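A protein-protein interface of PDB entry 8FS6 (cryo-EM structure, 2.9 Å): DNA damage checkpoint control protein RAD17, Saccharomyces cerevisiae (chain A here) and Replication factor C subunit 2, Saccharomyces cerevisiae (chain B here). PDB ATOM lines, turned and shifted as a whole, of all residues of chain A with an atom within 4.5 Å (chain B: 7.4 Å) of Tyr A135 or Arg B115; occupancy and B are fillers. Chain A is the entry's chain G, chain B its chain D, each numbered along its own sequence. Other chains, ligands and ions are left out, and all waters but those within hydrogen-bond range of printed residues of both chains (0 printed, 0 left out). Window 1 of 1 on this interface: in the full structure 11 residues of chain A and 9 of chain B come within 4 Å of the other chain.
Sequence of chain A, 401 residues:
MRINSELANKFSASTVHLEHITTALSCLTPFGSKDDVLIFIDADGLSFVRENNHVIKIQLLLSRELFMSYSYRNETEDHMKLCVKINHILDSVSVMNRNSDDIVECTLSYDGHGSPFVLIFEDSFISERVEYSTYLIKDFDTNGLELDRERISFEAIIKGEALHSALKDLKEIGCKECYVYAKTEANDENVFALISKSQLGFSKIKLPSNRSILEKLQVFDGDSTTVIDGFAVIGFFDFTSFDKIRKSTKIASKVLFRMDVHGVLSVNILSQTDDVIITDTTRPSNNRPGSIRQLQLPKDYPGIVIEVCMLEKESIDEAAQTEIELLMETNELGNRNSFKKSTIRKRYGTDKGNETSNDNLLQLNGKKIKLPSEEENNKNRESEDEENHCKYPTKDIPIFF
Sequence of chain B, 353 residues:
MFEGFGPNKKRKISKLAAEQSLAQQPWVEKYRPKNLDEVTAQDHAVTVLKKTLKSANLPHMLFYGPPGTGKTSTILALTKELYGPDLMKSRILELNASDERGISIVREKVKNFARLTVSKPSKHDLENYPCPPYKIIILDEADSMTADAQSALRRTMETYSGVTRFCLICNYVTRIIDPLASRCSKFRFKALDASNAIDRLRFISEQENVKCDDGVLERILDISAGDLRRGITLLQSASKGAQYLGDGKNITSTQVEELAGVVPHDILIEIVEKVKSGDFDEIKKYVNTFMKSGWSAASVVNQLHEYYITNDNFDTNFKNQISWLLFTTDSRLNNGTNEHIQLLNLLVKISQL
The guanidinium group (NH2) of Arg B115 is in hydrogen-bond range of the side-chain sulfur (SG) of Cys A83, at 3.6 Å. N of Leu A136 is in hydrogen-bond range of O of Arg B115 (2.6 Å). The side-chain hydroxyl of Thr B117 sits at hydrogen-bond distance from the backbone carbonyl oxygen of Thr A134 (2.4 Å).
ND2 of Asn B112 sits close to O of Glu B108, 3.3 Å away. OH of Tyr B160 is in hydrogen-bond range of NZ of Lys B111 (3.1 Å). O of Leu B116 lies within hydrogen-bond range of NZ of Lys B135 (2.7 Å). N of Lys B135 lies within hydrogen-bond range of O of Val B163 (3.1 Å). The backbone carbonyl oxygen (O) of Cys A83 is in hydrogen-bond range of the backbone NH (N) of Tyr A135 (2.6 Å).
Leu B116 touches Ser A133. Thr A134 touches Leu B116 (O to CD2, 3.3 Å). Tyr A135 touches Asn B112. Arg B115 touches Tyr A135 (O to CA, 3.5 Å). CD2 of Tyr A135 touches N of Leu B116 (3.9 Å). CD1 of Tyr B160 touches CD2 of Leu A136, 3.9 Å away. Val B163 touches Leu A136 (CG2 to CD2, 3.8 Å). NZ of Lys A138 touches NZ of Lys B111, 3.7 Å away. NH1 of Arg B115 touches CD of Lys A138 (3.4 Å). Tyr B160 touches Lys A138.
Of the printed residues of chain B, Ser A133 touches Leu B116 (3.3 Å). Of chain B, only Asn B112 (3.3 Å), Arg B115 (3.5 Å) and Leu B116 (3.9 Å) come within 4 Å of Tyr A135. Printed residues of chain B within 4 Å of Leu A136: Arg B115, Tyr B160 and Val B163. Printed residues of chain B within 4 Å of Lys A138: Lys B111, Arg B115 and Tyr B160. Printed residues of chain A within 4 Å of Lys B111: Lys A138. Of chain A, only Cys A83, Tyr A135, Leu A136 and Lys A138 come within 4 Å of Arg B115. Of the printed residues of chain A, Thr B117 touches Thr A134. Val B118 touches none of the printed residues of chain A. The nearest printed residue of chain B that does not touch Leu A136 is Thr B117 (4.2 Å).
Printed residues of chain B that touch a printed residue of chain A: Lys B111, Asn B112, Arg B115, Leu B116, Thr B117, Tyr B160 and Val B163. Hydrophobic or aromatic side chains of chain B that line the printed part of chain A: Leu B116, Tyr B160 and Val B163. Among the printed residues, no Asp or Glu carboxylate lies within 4 Å of a Lys or Arg side-chain nitrogen of the other chain.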
ATOM      1  N   CYS A  83      26.778   1.063  -6.708  1.00  0.00           N
ATOM      2  CA  CYS A  83      27.773   0.983  -7.774  1.00  0.00           C
ATOM      3  C   CYS A  83      28.947   1.894  -7.428  1.00  0.00           C
ATOM      4  O   CYS A  83      28.778   3.112  -7.308  1.00  0.00           O
ATOM      5  CB  CYS A  83      27.151   1.370  -9.115  1.00  0.00           C
ATOM      6  SG  CYS A  83      28.327   1.659 -10.446  1.00  0.00           S
ATOM      7  N   VAL A  84      30.134   1.303  -7.269  1.00  0.00           N
ATOM      8  CA  VAL A  84      31.348   2.035  -6.931  1.00  0.00           C
ATOM      9  C   VAL A  84      32.488   1.546  -7.817  1.00  0.00           C
ATOM     10  O   VAL A  84      32.410   0.488  -8.443  1.00  0.00           O
ATOM     11  CB  VAL A  84      31.730   1.887  -5.440  1.00  0.00           C
ATOM     12  CG1 VAL A  84      30.691   2.553  -4.548  1.00  0.00           C
ATOM     13  CG2 VAL A  84      31.890   0.419  -5.077  1.00  0.00           C
ATOM     14  N   LYS A  85      33.556   2.342  -7.865  1.00  0.00           N
ATOM     15  CA  LYS A  85      34.744   1.967  -8.622  1.00  0.00           C
ATOM     16  C   LYS A  85      35.520   0.867  -7.903  1.00  0.00           C
ATOM     17  O   LYS A  85      35.775   0.942  -6.700  1.00  0.00           O
ATOM     18  CB  LYS A  85      35.645   3.183  -8.839  1.00  0.00           C
ATOM     19  CG  LYS A  85      34.955   4.360  -9.509  1.00  0.00           C
ATOM     20  CD  LYS A  85      34.330   3.956 -10.834  1.00  0.00           C
ATOM     21  CE  LYS A  85      33.709   5.151 -11.536  1.00  0.00           C
ATOM     22  NZ  LYS A  85      33.033   4.762 -12.805  1.00  0.00           N
ATOM     23  N   SER A 133      31.674   7.114  -2.473  1.00  0.00           N
ATOM     24  CA  SER A 133      30.414   7.640  -2.977  1.00  0.00           C
ATOM     25  C   SER A 133      29.900   6.752  -4.104  1.00  0.00           C
ATOM     26  O   SER A 133      30.624   6.463  -5.060  1.00  0.00           O
ATOM     27  CB  SER A 133      30.592   9.075  -3.467  1.00  0.00           C
ATOM     28  OG  SER A 133      31.443   9.119  -4.598  1.00  0.00           O
ATOM     29  N   THR A 134      28.646   6.323  -3.989  1.00  0.00           N
ATOM     30  CA  THR A 134      28.065   5.413  -4.961  1.00  0.00           C
ATOM     31  C   THR A 134      27.667   6.157  -6.233  1.00  0.00           C
ATOM     32  O   THR A 134      27.436   7.368  -6.234  1.00  0.00           O
ATOM     33  CB  THR A 134      26.849   4.698  -4.372  1.00  0.00           C
ATOM     34  OG1 THR A 134      25.819   5.655  -4.094  1.00  0.00           O
ATOM     35  CG2 THR A 134      27.229   3.983  -3.085  1.00  0.00           C
ATOM     36  N   TYR A 135      27.586   5.405  -7.326  1.00  0.00           N
ATOM     37  CA  TYR A 135      27.202   5.929  -8.626  1.00  0.00           C
ATOM     38  C   TYR A 135      25.810   5.439  -9.000  1.00  0.00           C
ATOM     39  O   TYR A 135      25.277   4.497  -8.407  1.00  0.00           O
ATOM     40  CB  TYR A 135      28.208   5.514  -9.705  1.00  0.00           C
ATOM     41  CG  TYR A 135      29.532   6.237  -9.625  1.00  0.00           C
ATOM     42  CD1 TYR A 135      30.567   5.747  -8.841  1.00  0.00           C
ATOM     43  CD2 TYR A 135      29.747   7.409 -10.338  1.00  0.00           C
ATOM     44  CE1 TYR A 135      31.780   6.406  -8.765  1.00  0.00           C
ATOM     45  CE2 TYR A 135      30.956   8.073 -10.270  1.00  0.00           C
ATOM     46  CZ  TYR A 135      31.968   7.568  -9.482  1.00  0.00           C
ATOM     47  OH  TYR A 135      33.173   8.228  -9.413  1.00  0.00           O
ATOM     48  N   LEU A 136      25.224   6.099  -9.996  1.00  0.00           N
ATOM     49  CA  LEU A 136      23.911   5.701 -10.485  1.00  0.00           C
ATOM     50  C   LEU A 136      23.990   4.339 -11.164  1.00  0.00           C
ATOM     51  O   LEU A 136      24.943   4.042 -11.889  1.00  0.00           O
ATOM     52  CB  LEU A 136      23.366   6.747 -11.457  1.00  0.00           C
ATOM     53  CG  LEU A 136      21.921   6.562 -11.923  1.00  0.00           C
ATOM     54  CD1 LEU A 136      20.976   6.499 -10.732  1.00  0.00           C
ATOM     55  CD2 LEU A 136      21.517   7.677 -12.874  1.00  0.00           C
ATOM     56  N   ILE A 137      22.978   3.507 -10.919  1.00  0.00           N
ATOM     57  CA  ILE A 137      22.980   2.147 -11.445  1.00  0.00           C
ATOM     58  C   ILE A 137      22.710   2.177 -12.941  1.00  0.00           C
ATOM     59  O   ILE A 137      21.724   2.766 -13.402  1.00  0.00           O
ATOM     60  CB  ILE A 137      21.940   1.288 -10.710  1.00  0.00           C
ATOM     61  CG1 ILE A 137      22.107   1.427  -9.195  1.00  0.00           C
ATOM     62  CG2 ILE A 137      22.049  -0.166 -11.143  1.00  0.00           C
ATOM     63  CD1 ILE A 137      23.361   0.779  -8.654  1.00  0.00           C
ATOM     64  N   LYS A 138      23.590   1.541 -13.710  1.00  0.00           N
ATOM     65  CA  LYS A 138      23.383   1.419 -15.144  1.00  0.00           C
ATOM     66  C   LYS A 138      22.216   0.482 -15.434  1.00  0.00           C
ATOM     67  O   LYS A 138      21.967  -0.482 -14.706  1.00  0.00           O
ATOM     68  CB  LYS A 138      24.651   0.910 -15.830  1.00  0.00           C
ATOM     69  CG  LYS A 138      24.908   1.528 -17.196  1.00  0.00           C
ATOM     70  CD  LYS A 138      25.795   2.758 -17.088  1.00  0.00           C
ATOM     71  CE  LYS A 138      26.703   2.895 -18.298  1.00  0.00           C
ATOM     72  NZ  LYS A 138      27.680   4.007 -18.136  1.00  0.00           N
ATOM     73  N   GLU B 108      35.562  11.899 -18.790  1.00  0.00           N
ATOM     74  CA  GLU B 108      35.753  11.247 -17.498  1.00  0.00           C
ATOM     75  C   GLU B 108      35.192  12.052 -16.330  1.00  0.00           C
ATOM     76  O   GLU B 108      34.310  11.556 -15.627  1.00  0.00           O
ATOM     77  CB  GLU B 108      37.238  10.901 -17.256  1.00  0.00           C
ATOM     78  CG  GLU B 108      38.236  12.053 -17.283  1.00  0.00           C
ATOM     79  CD  GLU B 108      38.724  12.439 -15.900  1.00  0.00           C
ATOM     80  OE1 GLU B 108      38.073  12.051 -14.907  1.00  0.00           O
ATOM     81  OE2 GLU B 108      39.759  13.132 -15.806  1.00  0.00           O
ATOM     82  N   LYS B 109      35.639  13.293 -16.115  1.00  0.00           N
ATOM     83  CA  LYS B 109      35.283  14.001 -14.887  1.00  0.00           C
ATOM     84  C   LYS B 109      33.816  14.417 -14.887  1.00  0.00           C
ATOM     85  O   LYS B 109      33.087  14.170 -13.917  1.00  0.00           O
ATOM     86  CB  LYS B 109      36.191  15.218 -14.707  1.00  0.00           C
ATOM     87  CG  LYS B 109      35.626  16.298 -13.799  1.00  0.00           C
ATOM     88  CD  LYS B 109      36.723  17.222 -13.295  1.00  0.00           C
ATOM     89  CE  LYS B 109      36.274  17.999 -12.069  1.00  0.00           C
ATOM     90  NZ  LYS B 109      37.383  18.186 -11.092  1.00  0.00           N
ATOM     91  N   VAL B 110      33.364  15.043 -15.977  1.00  0.00           N
ATOM     92  CA  VAL B 110      31.975  15.486 -16.064  1.00  0.00           C
ATOM     93  C   VAL B 110      31.035  14.288 -16.070  1.00  0.00           C
ATOM     94  O   VAL B 110      29.986  14.298 -15.414  1.00  0.00           O
ATOM     95  CB  VAL B 110      31.776  16.373 -17.306  1.00  0.00           C
ATOM     96  CG1 VAL B 110      30.325  16.819 -17.422  1.00  0.00           C
ATOM     97  CG2 VAL B 110      32.705  17.577 -17.252  1.00  0.00           C
ATOM     98  N   LYS B 111      31.402  13.234 -16.804  1.00  0.00           N
ATOM     99  CA  LYS B 111      30.561  12.043 -16.863  1.00  0.00           C
ATOM    100  C   LYS B 111      30.468  11.355 -15.506  1.00  0.00           C
ATOM    101  O   LYS B 111      29.393  10.884 -15.118  1.00  0.00           O
ATOM    102  CB  LYS B 111      31.095  11.076 -17.920  1.00  0.00           C
ATOM    103  CG  LYS B 111      30.100  10.001 -18.325  1.00  0.00           C
ATOM    104  CD  LYS B 111      30.680   9.074 -19.378  1.00  0.00           C
ATOM    105  CE  LYS B 111      29.608   8.166 -19.957  1.00  0.00           C
ATOM    106  NZ  LYS B 111      28.852   7.452 -18.891  1.00  0.00           N
ATOM    107  N   ASN B 112      31.578  11.291 -14.763  1.00  0.00           N
ATOM    108  CA  ASN B 112      31.548  10.659 -13.450  1.00  0.00           C
ATOM    109  C   ASN B 112      30.788  11.501 -12.436  1.00  0.00           C
ATOM    110  O   ASN B 112      30.125  10.948 -11.551  1.00  0.00           O
ATOM    111  CB  ASN B 112      32.972  10.389 -12.965  1.00  0.00           C
ATOM    112  CG  ASN B 112      33.613   9.212 -13.671  1.00  0.00           C
ATOM    113  OD1 ASN B 112      32.940   8.446 -14.361  1.00  0.00           O
ATOM    114  ND2 ASN B 112      34.921   9.060 -13.503  1.00  0.00           N
ATOM    115  N   PHE B 113      30.874  12.832 -12.535  1.00  0.00           N
ATOM    116  CA  PHE B 113      30.067  13.669 -11.654  1.00  0.00           C
ATOM    117  C   PHE B 113      28.583  13.548 -11.978  1.00  0.00           C
ATOM    118  O   PHE B 113      27.750  13.555 -11.067  1.00  0.00           O
ATOM    119  CB  PHE B 113      30.513  15.128 -11.738  1.00  0.00           C
ATOM    120  CG  PHE B 113      29.887  16.010 -10.692  1.00  0.00           C
ATOM    121  CD1 PHE B 113      30.441  16.105  -9.426  1.00  0.00           C
ATOM    122  CD2 PHE B 113      28.741  16.736 -10.972  1.00  0.00           C
ATOM    123  CE1 PHE B 113      29.867  16.910  -8.461  1.00  0.00           C
ATOM    124  CE2 PHE B 113      28.162  17.543 -10.010  1.00  0.00           C
ATOM    125  CZ  PHE B 113      28.726  17.631  -8.754  1.00  0.00           C
ATOM    126  N   ALA B 114      28.235  13.440 -13.264  1.00  0.00           N
ATOM    127  CA  ALA B 114      26.840  13.235 -13.636  1.00  0.00           C
ATOM    128  C   ALA B 114      26.336  11.867 -13.193  1.00  0.00           C
ATOM    129  O   ALA B 114      25.170  11.734 -12.805  1.00  0.00           O
ATOM    130  CB  ALA B 114      26.668  13.399 -15.146  1.00  0.00           C
ATOM    131  N   ARG B 115      27.195  10.845 -13.244  1.00  0.00           N
ATOM    132  CA  ARG B 115      26.810   9.515 -12.788  1.00  0.00           C
ATOM    133  C   ARG B 115      26.700   9.430 -11.273  1.00  0.00           C
ATOM    134  O   ARG B 115      26.121   8.466 -10.760  1.00  0.00           O
ATOM    135  CB  ARG B 115      27.818   8.476 -13.283  1.00  0.00           C
ATOM    136  CG  ARG B 115      27.686   8.126 -14.753  1.00  0.00           C
ATOM    137  CD  ARG B 115      28.675   7.040 -15.151  1.00  0.00           C
ATOM    138  NE  ARG B 115      28.779   5.992 -14.143  1.00  0.00           N
ATOM    139  CZ  ARG B 115      27.885   5.028 -13.965  1.00  0.00           C
ATOM    140  NH1 ARG B 115      26.799   4.944 -14.716  1.00  0.00           N
ATOM    141  NH2 ARG B 115      28.087   4.124 -13.010  1.00  0.00           N
ATOM    142  N   LEU B 116      27.247  10.406 -10.551  1.00  0.00           N
ATOM    143  CA  LEU B 116      27.221  10.369  -9.096  1.00  0.00           C
ATOM    144  C   LEU B 116      25.796  10.512  -8.577  1.00  0.00           C
ATOM    145  O   LEU B 116      25.005  11.308  -9.091  1.00  0.00           O
ATOM    146  CB  LEU B 116      28.103  11.479  -8.525  1.00  0.00           C
ATOM    147  CG  LEU B 116      29.426  11.027  -7.908  1.00  0.00           C
ATOM    148  CD1 LEU B 116      30.309  12.224  -7.589  1.00  0.00           C
ATOM    149  CD2 LEU B 116      29.164  10.202  -6.664  1.00  0.00           C
ATOM    150  N   THR B 117      25.472   9.730  -7.552  1.00  0.00           N
ATOM    151  CA  THR B 117      24.157   9.804  -6.938  1.00  0.00           C
ATOM    152  C   THR B 117      23.987  11.124  -6.194  1.00  0.00           C
ATOM    153  O   THR B 117      24.956  11.738  -5.741  1.00  0.00           O
ATOM    154  CB  THR B 117      23.943   8.634  -5.979  1.00  0.00           C
ATOM    155  OG1 THR B 117      25.213   8.129  -5.547  1.00  0.00           O
ATOM    156  CG2 THR B 117      23.167   7.518  -6.663  1.00  0.00           C
ATOM    157  N   VAL B 118      22.733  11.561  -6.078  1.00  0.00           N
ATOM    158  CA  VAL B 118      22.435  12.815  -5.400  1.00  0.00           C
ATOM    159  C   VAL B 118      22.697  12.656  -3.908  1.00  0.00           C
ATOM    160  O   VAL B 118      22.185  11.730  -3.266  1.00  0.00           O
ATOM    161  CB  VAL B 118      20.986  13.240  -5.674  1.00  0.00           C
ATOM    162  CG1 VAL B 118      20.557  14.337  -4.714  1.00  0.00           C
ATOM    163  CG2 VAL B 118      20.834  13.697  -7.116  1.00  0.00           C
ATOM    164  N   LYS B 135      21.765  17.611  -9.029  1.00  0.00           N
ATOM    165  CA  LYS B 135      22.936  18.467  -8.941  1.00  0.00           C
ATOM    166  C   LYS B 135      23.075  19.283 -10.218  1.00  0.00           C
ATOM    167  O   LYS B 135      22.477  18.969 -11.251  1.00  0.00           O
ATOM    168  CB  LYS B 135      24.205  17.644  -8.693  1.00  0.00           C
ATOM    169  CG  LYS B 135      23.975  16.393  -7.862  1.00  0.00           C
ATOM    170  CD  LYS B 135      25.243  15.564  -7.755  1.00  0.00           C
ATOM    171  CE  LYS B 135      25.620  14.965  -9.096  1.00  0.00           C
ATOM    172  NZ  LYS B 135      24.635  13.947  -9.547  1.00  0.00           N
ATOM    173  N   ILE B 137      25.784  21.102 -12.922  1.00  0.00           N
ATOM    174  CA  ILE B 137      27.126  21.205 -13.482  1.00  0.00           C
ATOM    175  C   ILE B 137      27.184  22.510 -14.261  1.00  0.00           C
ATOM    176  O   ILE B 137      26.551  22.644 -15.316  1.00  0.00           O
ATOM    177  CB  ILE B 137      27.469  20.007 -14.378  1.00  0.00           C
ATOM    178  CG1 ILE B 137      27.327  18.699 -13.599  1.00  0.00           C
ATOM    179  CG2 ILE B 137      28.874  20.152 -14.943  1.00  0.00           C
ATOM    180  CD1 ILE B 137      27.801  17.479 -14.361  1.00  0.00           C
ATOM    181  N   THR B 156      25.433  13.039 -22.286  1.00  0.00           N
ATOM    182  CA  THR B 156      25.596  13.176 -20.843  1.00  0.00           C
ATOM    183  C   THR B 156      24.487  14.023 -20.228  1.00  0.00           C
ATOM    184  O   THR B 156      24.016  13.718 -19.126  1.00  0.00           O
ATOM    185  CB  THR B 156      26.966  13.773 -20.520  1.00  0.00           C
ATOM    186  OG1 THR B 156      27.976  13.089 -21.273  1.00  0.00           O
ATOM    187  CG2 THR B 156      27.274  13.630 -19.038  1.00  0.00           C
ATOM    188  N   TYR B 160      21.510  11.304 -17.956  1.00  0.00           N
ATOM    189  CA  TYR B 160      21.455  11.610 -16.531  1.00  0.00           C
ATOM    190  C   TYR B 160      20.753  12.940 -16.275  1.00  0.00           C
ATOM    191  O   TYR B 160      21.096  13.674 -15.348  1.00  0.00           O
ATOM    192  CB  TYR B 160      22.859  11.623 -15.931  1.00  0.00           C
ATOM    193  CG  TYR B 160      23.717  10.465 -16.380  1.00  0.00           C
ATOM    194  CD1 TYR B 160      23.435   9.167 -15.975  1.00  0.00           C
ATOM    195  CD2 TYR B 160      24.813  10.668 -17.209  1.00  0.00           C
ATOM    196  CE1 TYR B 160      24.220   8.104 -16.382  1.00  0.00           C
ATOM    197  CE2 TYR B 160      25.604   9.613 -17.621  1.00  0.00           C
ATOM    198  CZ  TYR B 160      25.303   8.333 -17.203  1.00  0.00           C
ATOM    199  OH  TYR B 160      26.086   7.278 -17.612  1.00  0.00           O
ATOM    200  N   VAL B 163      19.228  13.260 -12.749  1.00  0.00           N
ATOM    201  CA  VAL B 163      20.106  13.163 -11.589  1.00  0.00           C
ATOM    202  C   VAL B 163      21.001  14.396 -11.551  1.00  0.00           C
ATOM    203  O   VAL B 163      21.369  14.882 -10.474  1.00  0.00           O
ATOM    204  CB  VAL B 163      20.919  11.851 -11.636  1.00  0.00           C
ATOM    205  CG1 VAL B 163      22.252  11.979 -10.910  1.00  0.00           C
ATOM    206  CG2 VAL B 163      20.103  10.705 -11.056  1.00  0.00           C
ATOM    207  N   THR B 164      21.306  14.950 -12.723  1.00  0.00           N
ATOM    208  CA  THR B 164      22.161  16.121 -12.829  1.00  0.00           C
ATOM    209  C   THR B 164      21.554  17.121 -13.804  1.00  0.00           C
ATOM    210  O   THR B 164      20.741  16.774 -14.664  1.00  0.00           O
ATOM    211  CB  THR B 164      23.589  15.744 -13.267  1.00  0.00           C
ATOM    212  OG1 THR B 164      24.511  16.739 -12.805  1.00  0.00           O
ATOM    213  CG2 THR B 164      23.689  15.633 -14.782  1.00  0.00           C
